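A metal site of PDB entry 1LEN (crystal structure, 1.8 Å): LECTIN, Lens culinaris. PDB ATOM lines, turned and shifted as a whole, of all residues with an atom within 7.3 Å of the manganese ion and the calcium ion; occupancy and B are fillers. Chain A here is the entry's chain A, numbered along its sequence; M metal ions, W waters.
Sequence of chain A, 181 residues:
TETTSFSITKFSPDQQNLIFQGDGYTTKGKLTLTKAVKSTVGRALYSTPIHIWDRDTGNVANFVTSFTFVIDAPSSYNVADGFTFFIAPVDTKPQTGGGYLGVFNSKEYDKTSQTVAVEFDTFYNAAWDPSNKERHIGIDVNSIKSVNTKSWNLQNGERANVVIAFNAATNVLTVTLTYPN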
ATOM      1  N   ASP A  81     -31.033   7.431 -19.100  1.00  0.00           N
ATOM      2  CA  ASP A  81     -30.315   6.536 -20.002  1.00  0.00           C
ATOM      3  C   ASP A  81     -30.770   6.799 -21.443  1.00  0.00           C
ATOM      4  O   ASP A  81     -30.071   6.591 -22.401  1.00  0.00           O
ATOM      5  CB  ASP A  81     -30.645   5.054 -19.701  1.00  0.00           C
ATOM      6  CG  ASP A  81     -29.491   4.447 -18.859  1.00  0.00           C
ATOM      7  OD1 ASP A  81     -28.421   4.274 -19.405  1.00  0.00           O
ATOM      8  OD2 ASP A  81     -29.708   4.242 -17.657  1.00  0.00           O
ATOM      9  N   GLY A  82     -32.020   7.301 -21.459  1.00  0.00           N
ATOM     10  CA  GLY A  82     -32.543   7.571 -22.817  1.00  0.00           C
ATOM     11  C   GLY A  82     -34.030   7.295 -22.953  1.00  0.00           C
ATOM     12  O   GLY A  82     -34.710   6.858 -22.055  1.00  0.00           O
ATOM     13  N   GLY A  98     -32.207   0.440 -17.274  1.00  0.00           N
ATOM     14  CA  GLY A  98     -30.967   1.163 -17.445  1.00  0.00           C
ATOM     15  C   GLY A  98     -30.596   1.264 -18.896  1.00  0.00           C
ATOM     16  O   GLY A  98     -31.456   1.671 -19.642  1.00  0.00           O
ATOM     17  N   GLY A  99     -29.409   0.964 -19.322  1.00  0.00           N
ATOM     18  CA  GLY A  99     -28.897   1.042 -20.678  1.00  0.00           C
ATOM     19  C   GLY A  99     -29.720   0.212 -21.669  1.00  0.00           C
ATOM     20  O   GLY A  99     -29.579   0.485 -22.848  1.00  0.00           O
ATOM     21  N   TYR A 100     -30.545  -0.729 -21.275  1.00  0.00           N
ATOM     22  CA  TYR A 100     -31.343  -1.537 -22.195  1.00  0.00           C
ATOM     23  C   TYR A 100     -32.628  -0.865 -22.580  1.00  0.00           C
ATOM     24  O   TYR A 100     -33.334  -1.377 -23.427  1.00  0.00           O
ATOM     25  CB  TYR A 100     -31.558  -2.931 -21.730  1.00  0.00           C
ATOM     26  CG  TYR A 100     -30.264  -3.779 -21.729  1.00  0.00           C
ATOM     27  CD1 TYR A 100     -29.822  -4.488 -22.815  1.00  0.00           C
ATOM     28  CD2 TYR A 100     -29.611  -3.834 -20.512  1.00  0.00           C
ATOM     29  CE1 TYR A 100     -28.641  -5.234 -22.638  1.00  0.00           C
ATOM     30  CE2 TYR A 100     -28.464  -4.571 -20.332  1.00  0.00           C
ATOM     31  CZ  TYR A 100     -27.998  -5.279 -21.423  1.00  0.00           C
ATOM     32  OH  TYR A 100     -26.857  -5.987 -21.197  1.00  0.00           O
ATOM     33  N   LEU A 101     -32.909   0.265 -21.973  1.00  0.00           N
ATOM     34  CA  LEU A 101     -34.019   1.141 -22.243  1.00  0.00           C
ATOM     35  C   LEU A 101     -35.368   0.544 -21.971  1.00  0.00           C
ATOM     36  O   LEU A 101     -36.329   1.129 -22.489  1.00  0.00           O
ATOM     37  CB  LEU A 101     -33.963   1.739 -23.656  1.00  0.00           C
ATOM     38  CG  LEU A 101     -32.696   2.545 -23.892  1.00  0.00           C
ATOM     39  CD1 LEU A 101     -32.400   2.944 -25.340  1.00  0.00           C
ATOM     40  CD2 LEU A 101     -32.567   3.742 -22.985  1.00  0.00           C
ATOM     41  N   GLU A 119     -34.060   4.741 -30.777  1.00  0.00           N
ATOM     42  CA  GLU A 119     -33.591   5.275 -29.517  1.00  0.00           C
ATOM     43  C   GLU A 119     -32.958   6.633 -29.640  1.00  0.00           C
ATOM     44  O   GLU A 119     -32.415   7.044 -30.656  1.00  0.00           O
ATOM     45  CB  GLU A 119     -32.585   4.295 -28.873  1.00  0.00           C
ATOM     46  CG  GLU A 119     -31.418   4.174 -29.851  1.00  0.00           C
ATOM     47  CD  GLU A 119     -30.253   3.480 -29.232  1.00  0.00           C
ATOM     48  OE1 GLU A 119     -30.359   2.389 -28.677  1.00  0.00           O
ATOM     49  OE2 GLU A 119     -29.119   3.975 -29.232  1.00  0.00           O
ATOM     50  N   PHE A 120     -33.059   7.352 -28.575  1.00  0.00           N
ATOM     51  CA  PHE A 120     -32.545   8.701 -28.229  1.00  0.00           C
ATOM     52  C   PHE A 120     -31.792   8.482 -26.909  1.00  0.00           C
ATOM     53  O   PHE A 120     -32.222   8.520 -25.822  1.00  0.00           O
ATOM     54  CB  PHE A 120     -33.718   9.661 -28.074  1.00  0.00           C
ATOM     55  CG  PHE A 120     -34.553   9.725 -29.344  1.00  0.00           C
ATOM     56  CD1 PHE A 120     -34.191  10.605 -30.359  1.00  0.00           C
ATOM     57  CD2 PHE A 120     -35.674   8.886 -29.495  1.00  0.00           C
ATOM     58  CE1 PHE A 120     -34.944  10.649 -31.540  1.00  0.00           C
ATOM     59  CE2 PHE A 120     -36.431   8.937 -30.671  1.00  0.00           C
ATOM     60  CZ  PHE A 120     -36.061   9.824 -31.688  1.00  0.00           C
ATOM     61  N   ASP A 121     -30.576   8.012 -27.150  1.00  0.00           N
ATOM     62  CA  ASP A 121     -29.600   7.548 -26.170  1.00  0.00           C
ATOM     63  C   ASP A 121     -28.669   8.650 -25.697  1.00  0.00           C
ATOM     64  O   ASP A 121     -27.859   9.232 -26.375  1.00  0.00           O
ATOM     65  CB  ASP A 121     -28.781   6.390 -26.769  1.00  0.00           C
ATOM     66  CG  ASP A 121     -28.016   5.588 -25.733  1.00  0.00           C
ATOM     67  OD1 ASP A 121     -27.864   5.966 -24.563  1.00  0.00           O
ATOM     68  OD2 ASP A 121     -27.536   4.447 -25.975  1.00  0.00           O
ATOM     69  N   THR A 122     -28.831   8.940 -24.398  1.00  0.00           N
ATOM     70  CA  THR A 122     -28.130  10.004 -23.720  1.00  0.00           C
ATOM     71  C   THR A 122     -26.951   9.531 -22.905  1.00  0.00           C
ATOM     72  O   THR A 122     -26.274  10.435 -22.386  1.00  0.00           O
ATOM     73  CB  THR A 122     -29.103  10.790 -22.827  1.00  0.00           C
ATOM     74  OG1 THR A 122     -29.682   9.938 -21.845  1.00  0.00           O
ATOM     75  CG2 THR A 122     -30.197  11.375 -23.673  1.00  0.00           C
ATOM     76  N   PHE A 123     -26.668   8.282 -22.742  1.00  0.00           N
ATOM     77  CA  PHE A 123     -25.589   7.752 -21.887  1.00  0.00           C
ATOM     78  C   PHE A 123     -24.829   6.627 -22.560  1.00  0.00           C
ATOM     79  O   PHE A 123     -25.362   5.601 -23.016  1.00  0.00           O
ATOM     80  CB  PHE A 123     -26.186   7.281 -20.584  1.00  0.00           C
ATOM     81  CG  PHE A 123     -25.182   6.771 -19.566  1.00  0.00           C
ATOM     82  CD1 PHE A 123     -24.619   7.706 -18.688  1.00  0.00           C
ATOM     83  CD2 PHE A 123     -24.897   5.425 -19.503  1.00  0.00           C
ATOM     84  CE1 PHE A 123     -23.735   7.161 -17.766  1.00  0.00           C
ATOM     85  CE2 PHE A 123     -24.000   4.903 -18.568  1.00  0.00           C
ATOM     86  CZ  PHE A 123     -23.426   5.816 -17.707  1.00  0.00           C
ATOM     87  N   TYR A 124     -23.525   6.818 -22.614  1.00  0.00           N
ATOM     88  CA  TYR A 124     -22.568   5.916 -23.248  1.00  0.00           C
ATOM     89  C   TYR A 124     -22.383   4.625 -22.499  1.00  0.00           C
ATOM     90  O   TYR A 124     -21.768   4.643 -21.424  1.00  0.00           O
ATOM     91  CB  TYR A 124     -21.219   6.629 -23.375  1.00  0.00           C
ATOM     92  CG  TYR A 124     -20.138   5.708 -23.913  1.00  0.00           C
ATOM     93  CD1 TYR A 124     -20.189   5.316 -25.238  1.00  0.00           C
ATOM     94  CD2 TYR A 124     -19.107   5.277 -23.070  1.00  0.00           C
ATOM     95  CE1 TYR A 124     -19.196   4.490 -25.691  1.00  0.00           C
ATOM     96  CE2 TYR A 124     -18.136   4.438 -23.539  1.00  0.00           C
ATOM     97  CZ  TYR A 124     -18.178   4.035 -24.862  1.00  0.00           C
ATOM     98  OH  TYR A 124     -17.204   3.210 -25.394  1.00  0.00           O
ATOM     99  N   ASN A 125     -22.885   3.500 -22.985  1.00  0.00           N
ATOM    100  CA  ASN A 125     -22.641   2.172 -22.340  1.00  0.00           C
ATOM    101  C   ASN A 125     -21.485   1.555 -23.139  1.00  0.00           C
ATOM    102  O   ASN A 125     -21.630   1.336 -24.325  1.00  0.00           O
ATOM    103  CB  ASN A 125     -23.871   1.302 -22.486  1.00  0.00           C
ATOM    104  CG  ASN A 125     -25.021   1.978 -21.719  1.00  0.00           C
ATOM    105  OD1 ASN A 125     -25.790   2.840 -22.332  1.00  0.00           O
ATOM    106  ND2 ASN A 125     -25.093   1.635 -20.450  1.00  0.00           N
ATOM    107  N   ALA A 126     -20.351   1.416 -22.544  1.00  0.00           N
ATOM    108  CA  ALA A 126     -19.155   0.938 -23.219  1.00  0.00           C
ATOM    109  C   ALA A 126     -19.323  -0.381 -23.906  1.00  0.00           C
ATOM    110  O   ALA A 126     -18.658  -0.565 -24.961  1.00  0.00           O
ATOM    111  CB  ALA A 126     -17.971   0.938 -22.277  1.00  0.00           C
ATOM    112  N   TRP A 128     -21.637  -1.536 -25.822  1.00  0.00           N
ATOM    113  CA  TRP A 128     -22.198  -1.582 -27.197  1.00  0.00           C
ATOM    114  C   TRP A 128     -22.407  -0.213 -27.770  1.00  0.00           C
ATOM    115  O   TRP A 128     -22.750  -0.249 -28.960  1.00  0.00           O
ATOM    116  CB  TRP A 128     -23.563  -2.307 -27.131  1.00  0.00           C
ATOM    117  CG  TRP A 128     -24.523  -1.595 -26.160  1.00  0.00           C
ATOM    118  CD1 TRP A 128     -25.191  -0.448 -26.401  1.00  0.00           C
ATOM    119  CD2 TRP A 128     -24.875  -2.038 -24.876  1.00  0.00           C
ATOM    120  NE1 TRP A 128     -25.957  -0.158 -25.232  1.00  0.00           N
ATOM    121  CE2 TRP A 128     -25.741  -1.114 -24.345  1.00  0.00           C
ATOM    122  CE3 TRP A 128     -24.515  -3.145 -24.089  1.00  0.00           C
ATOM    123  CZ2 TRP A 128     -26.261  -1.253 -23.104  1.00  0.00           C
ATOM    124  CZ3 TRP A 128     -25.044  -3.253 -22.840  1.00  0.00           C
ATOM    125  CH2 TRP A 128     -25.933  -2.322 -22.314  1.00  0.00           C
ATOM    126  N   ASP A 129     -22.322   0.943 -27.157  1.00  0.00           N
ATOM    127  CA  ASP A 129     -22.614   2.232 -27.836  1.00  0.00           C
ATOM    128  C   ASP A 129     -21.451   2.670 -28.695  1.00  0.00           C
ATOM    129  O   ASP A 129     -20.363   2.180 -28.411  1.00  0.00           O
ATOM    130  CB  ASP A 129     -22.878   3.323 -26.760  1.00  0.00           C
ATOM    131  CG  ASP A 129     -24.290   3.210 -26.233  1.00  0.00           C
ATOM    132  OD1 ASP A 129     -25.129   2.828 -27.065  1.00  0.00           O
ATOM    133  OD2 ASP A 129     -24.694   3.478 -25.103  1.00  0.00           O
ATOM    134  N   PRO A 130     -21.676   3.570 -29.655  1.00  0.00           N
ATOM    135  CA  PRO A 130     -20.582   4.063 -30.503  1.00  0.00           C
ATOM    136  C   PRO A 130     -19.424   4.553 -29.673  1.00  0.00           C
ATOM    137  O   PRO A 130     -19.581   5.233 -28.662  1.00  0.00           O
ATOM    138  CB  PRO A 130     -21.257   5.166 -31.259  1.00  0.00           C
ATOM    139  CG  PRO A 130     -22.750   5.018 -31.171  1.00  0.00           C
ATOM    140  CD  PRO A 130     -22.988   4.119 -29.993  1.00  0.00           C
ATOM    141  N   GLU A 134     -20.444   9.783 -27.969  1.00  0.00           N
ATOM    142  CA  GLU A 134     -21.414  10.882 -28.169  1.00  0.00           C
ATOM    143  C   GLU A 134     -22.827  10.403 -27.941  1.00  0.00           C
ATOM    144  O   GLU A 134     -23.175   9.247 -28.116  1.00  0.00           O
ATOM    145  CB  GLU A 134     -21.269  11.385 -29.599  1.00  0.00           C
ATOM    146  CG  GLU A 134     -20.808  12.817 -29.580  1.00  0.00           C
ATOM    147  CD  GLU A 134     -19.883  13.134 -30.738  1.00  0.00           C
ATOM    148  OE1 GLU A 134     -18.674  12.870 -30.596  1.00  0.00           O
ATOM    149  OE2 GLU A 134     -20.280  13.665 -31.781  1.00  0.00           O
ATOM    150  N   HIS A 136     -26.676   9.887 -29.031  1.00  0.00           N
ATOM    151  CA  HIS A 136     -26.975   9.670 -30.460  1.00  0.00           C
ATOM    152  C   HIS A 136     -28.397   9.127 -30.659  1.00  0.00           C
ATOM    153  O   HIS A 136     -29.066   8.623 -29.774  1.00  0.00           O
ATOM    154  CB  HIS A 136     -26.026   8.505 -30.923  1.00  0.00           C
ATOM    155  CG  HIS A 136     -25.938   7.338 -29.947  1.00  0.00           C
ATOM    156  ND1 HIS A 136     -25.268   7.258 -28.742  1.00  0.00           N
ATOM    157  CD2 HIS A 136     -26.570   6.094 -30.058  1.00  0.00           C
ATOM    158  CE1 HIS A 136     -25.455   6.063 -28.129  1.00  0.00           C
ATOM    159  NE2 HIS A 136     -26.265   5.307 -28.935  1.00  0.00           N
ATOM    160  N   ILE A 137     -28.816   9.246 -31.910  1.00  0.00           N
ATOM    161  CA  ILE A 137     -30.109   8.643 -32.292  1.00  0.00           C
ATOM    162  C   ILE A 137     -29.806   7.265 -32.892  1.00  0.00           C
ATOM    163  O   ILE A 137     -28.815   7.159 -33.629  1.00  0.00           O
ATOM    164  CB  ILE A 137     -30.799   9.491 -33.353  1.00  0.00           C
ATOM    165  CG1 ILE A 137     -31.051  10.907 -32.817  1.00  0.00           C
ATOM    166  CG2 ILE A 137     -32.129   8.842 -33.753  1.00  0.00           C
ATOM    167  CD1 ILE A 137     -31.108  11.873 -34.002  1.00  0.00           C
ATOM    168  N   GLY A 138     -30.500   6.192 -32.661  1.00  0.00           N
ATOM    169  CA  GLY A 138     -30.096   4.942 -33.284  1.00  0.00           C
ATOM    170  C   GLY A 138     -31.294   4.112 -33.707  1.00  0.00           C
ATOM    171  O   GLY A 138     -32.398   4.314 -33.216  1.00  0.00           O
ATOM    172  N   ASP A 140     -32.630   0.275 -33.760  1.00  0.00           N
ATOM    173  CA  ASP A 140     -32.397  -0.970 -33.069  1.00  0.00           C
ATOM    174  C   ASP A 140     -33.325  -2.068 -33.529  1.00  0.00           C
ATOM    175  O   ASP A 140     -34.508  -1.829 -33.459  1.00  0.00           O
ATOM    176  CB  ASP A 140     -32.569  -0.804 -31.548  1.00  0.00           C
ATOM    177  CG  ASP A 140     -31.710   0.255 -30.902  1.00  0.00           C
ATOM    178  OD1 ASP A 140     -30.830   0.864 -31.487  1.00  0.00           O
ATOM    179  OD2 ASP A 140     -31.919   0.516 -29.714  1.00  0.00           O
ATOM    180  N   ILE A 144     -29.926  -4.115 -28.378  1.00  0.00           N
ATOM    181  CA  ILE A 144     -29.597  -2.786 -27.854  1.00  0.00           C
ATOM    182  C   ILE A 144     -28.495  -2.135 -28.651  1.00  0.00           C
ATOM    183  O   ILE A 144     -28.233  -0.960 -28.683  1.00  0.00           O
ATOM    184  CB  ILE A 144     -29.299  -2.804 -26.381  1.00  0.00           C
ATOM    185  CG1 ILE A 144     -29.465  -1.447 -25.723  1.00  0.00           C
ATOM    186  CG2 ILE A 144     -27.961  -3.434 -26.046  1.00  0.00           C
ATOM    187  CD1 ILE A 144     -30.771  -0.713 -25.928  1.00  0.00           C
ATOM    188  N   LYS A 145     -27.777  -2.980 -29.381  1.00  0.00           N
ATOM    189  CA  LYS A 145     -26.650  -2.537 -30.250  1.00  0.00           C
ATOM    190  C   LYS A 145     -27.236  -1.971 -31.547  1.00  0.00           C
ATOM    191  O   LYS A 145     -27.576  -2.820 -32.375  1.00  0.00           O
ATOM    192  CB  LYS A 145     -25.896  -3.850 -30.624  1.00  0.00           C
ATOM    193  CG  LYS A 145     -24.466  -3.609 -30.297  1.00  0.00           C
ATOM    194  CD  LYS A 145     -23.847  -3.024 -31.538  1.00  0.00           C
ATOM    195  CE  LYS A 145     -23.086  -4.195 -32.206  1.00  0.00           C
ATOM    196  NZ  LYS A 145     -23.172  -3.963 -33.655  1.00  0.00           N
ATOM    197  N   SER A 146     -27.406  -0.743 -31.849  1.00  0.00           N
ATOM    198  CA  SER A 146     -28.046  -0.214 -33.052  1.00  0.00           C
ATOM    199  C   SER A 146     -27.440  -0.665 -34.343  1.00  0.00           C
ATOM    200  O   SER A 146     -26.232  -0.733 -34.532  1.00  0.00           O
ATOM    201  CB  SER A 146     -28.035   1.320 -33.009  1.00  0.00           C
ATOM    202  OG  SER A 146     -28.381   1.759 -31.714  1.00  0.00           O
ATOM    203  N   THR A 149     -26.559   4.575 -36.275  1.00  0.00           N
ATOM    204  CA  THR A 149     -26.614   5.643 -35.279  1.00  0.00           C
ATOM    205  C   THR A 149     -26.214   6.971 -35.935  1.00  0.00           C
ATOM    206  O   THR A 149     -25.593   7.006 -36.978  1.00  0.00           O
ATOM    207  CB  THR A 149     -25.720   5.373 -34.095  1.00  0.00           C
ATOM    208  OG1 THR A 149     -24.348   5.425 -34.441  1.00  0.00           O
ATOM    209  CG2 THR A 149     -26.008   4.084 -33.417  1.00  0.00           C
HETATM  210 MN    MN M   1     -27.104   3.444 -28.078  1.00  0.00          MN
HETATM  211 CA    CA M   2     -26.647   4.015 -23.926  1.00  0.00          CA
HETATM  212  O   HOH W   1     -27.857   2.154 -24.518  1.00  0.00           O
HETATM  213  O   HOH W   2     -26.563   2.382 -29.833  1.00  0.00           O
HETATM  214  O   HOH W   3     -28.264   4.606 -22.314  1.00  0.00           O
HETATM  215  O   HOH W   4     -28.097   1.627 -27.402  1.00  0.00           O
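Four residues have an atom within 4 Å of the manganese ion: Glu 119, Asp 121, Asp 129 and His 136. The nearest printed residue that does not touch the manganese ion is Ser 146 (4.2 Å).
The backbone carbonyl oxygen (O) of Glu 134 sits at hydrogen-bond distance from a ring nitrogen (ND1) of His 136 (3.0 Å). OG of Ser 146 lies close to OE2 of Glu 119 (3.4 Å). The side-chain carboxylate (OE1) of Glu 119 lies close to the side-chain carboxylate (OD2) of Asp 140 (2.6 Å). O of Glu 119 is in hydrogen-bond range of N of Gly 138 (2.9 Å).
The calcium ion is bound by OD1 of Asn 125 (2.2 Å), O of Phe 123 (2.2 Å), OD2 of Asp 121 (2.3 Å), water W1 (2.3 Å), OD2 of Asp 129 (2.3 Å), water W3 (2.4 Å) and OD1 of Asp 121 (2.4 Å).
Water W4 lies within hydrogen-bond range of OE1 of Glu 119 (2.7 Å) and O of Ile 144 (2.9 Å). Water W1 bridges the backbone carbonyl oxygen of Gly 99 and the indole nitrogen of Trp 128.
Four residues have an atom within 4 Å of the calcium ion: Asp 121, Phe 123, Asn 125 and Asp 129. Along chain A the residues within 4 Å of the calcium ion span positions 121 to 129.
The manganese ion is bound by water W2 (2.1 Å), water W4 (2.2 Å), a ring nitrogen (NE2) of His 136 (2.2 Å), the side-chain carboxylate of Asp 129 (2.3 Å), the side-chain carboxylate of Asp 121 (2.4 Å) and the side-chain carboxylate of Glu 119 (2.4 Å). The manganese ion has six donor atoms within binding distance.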
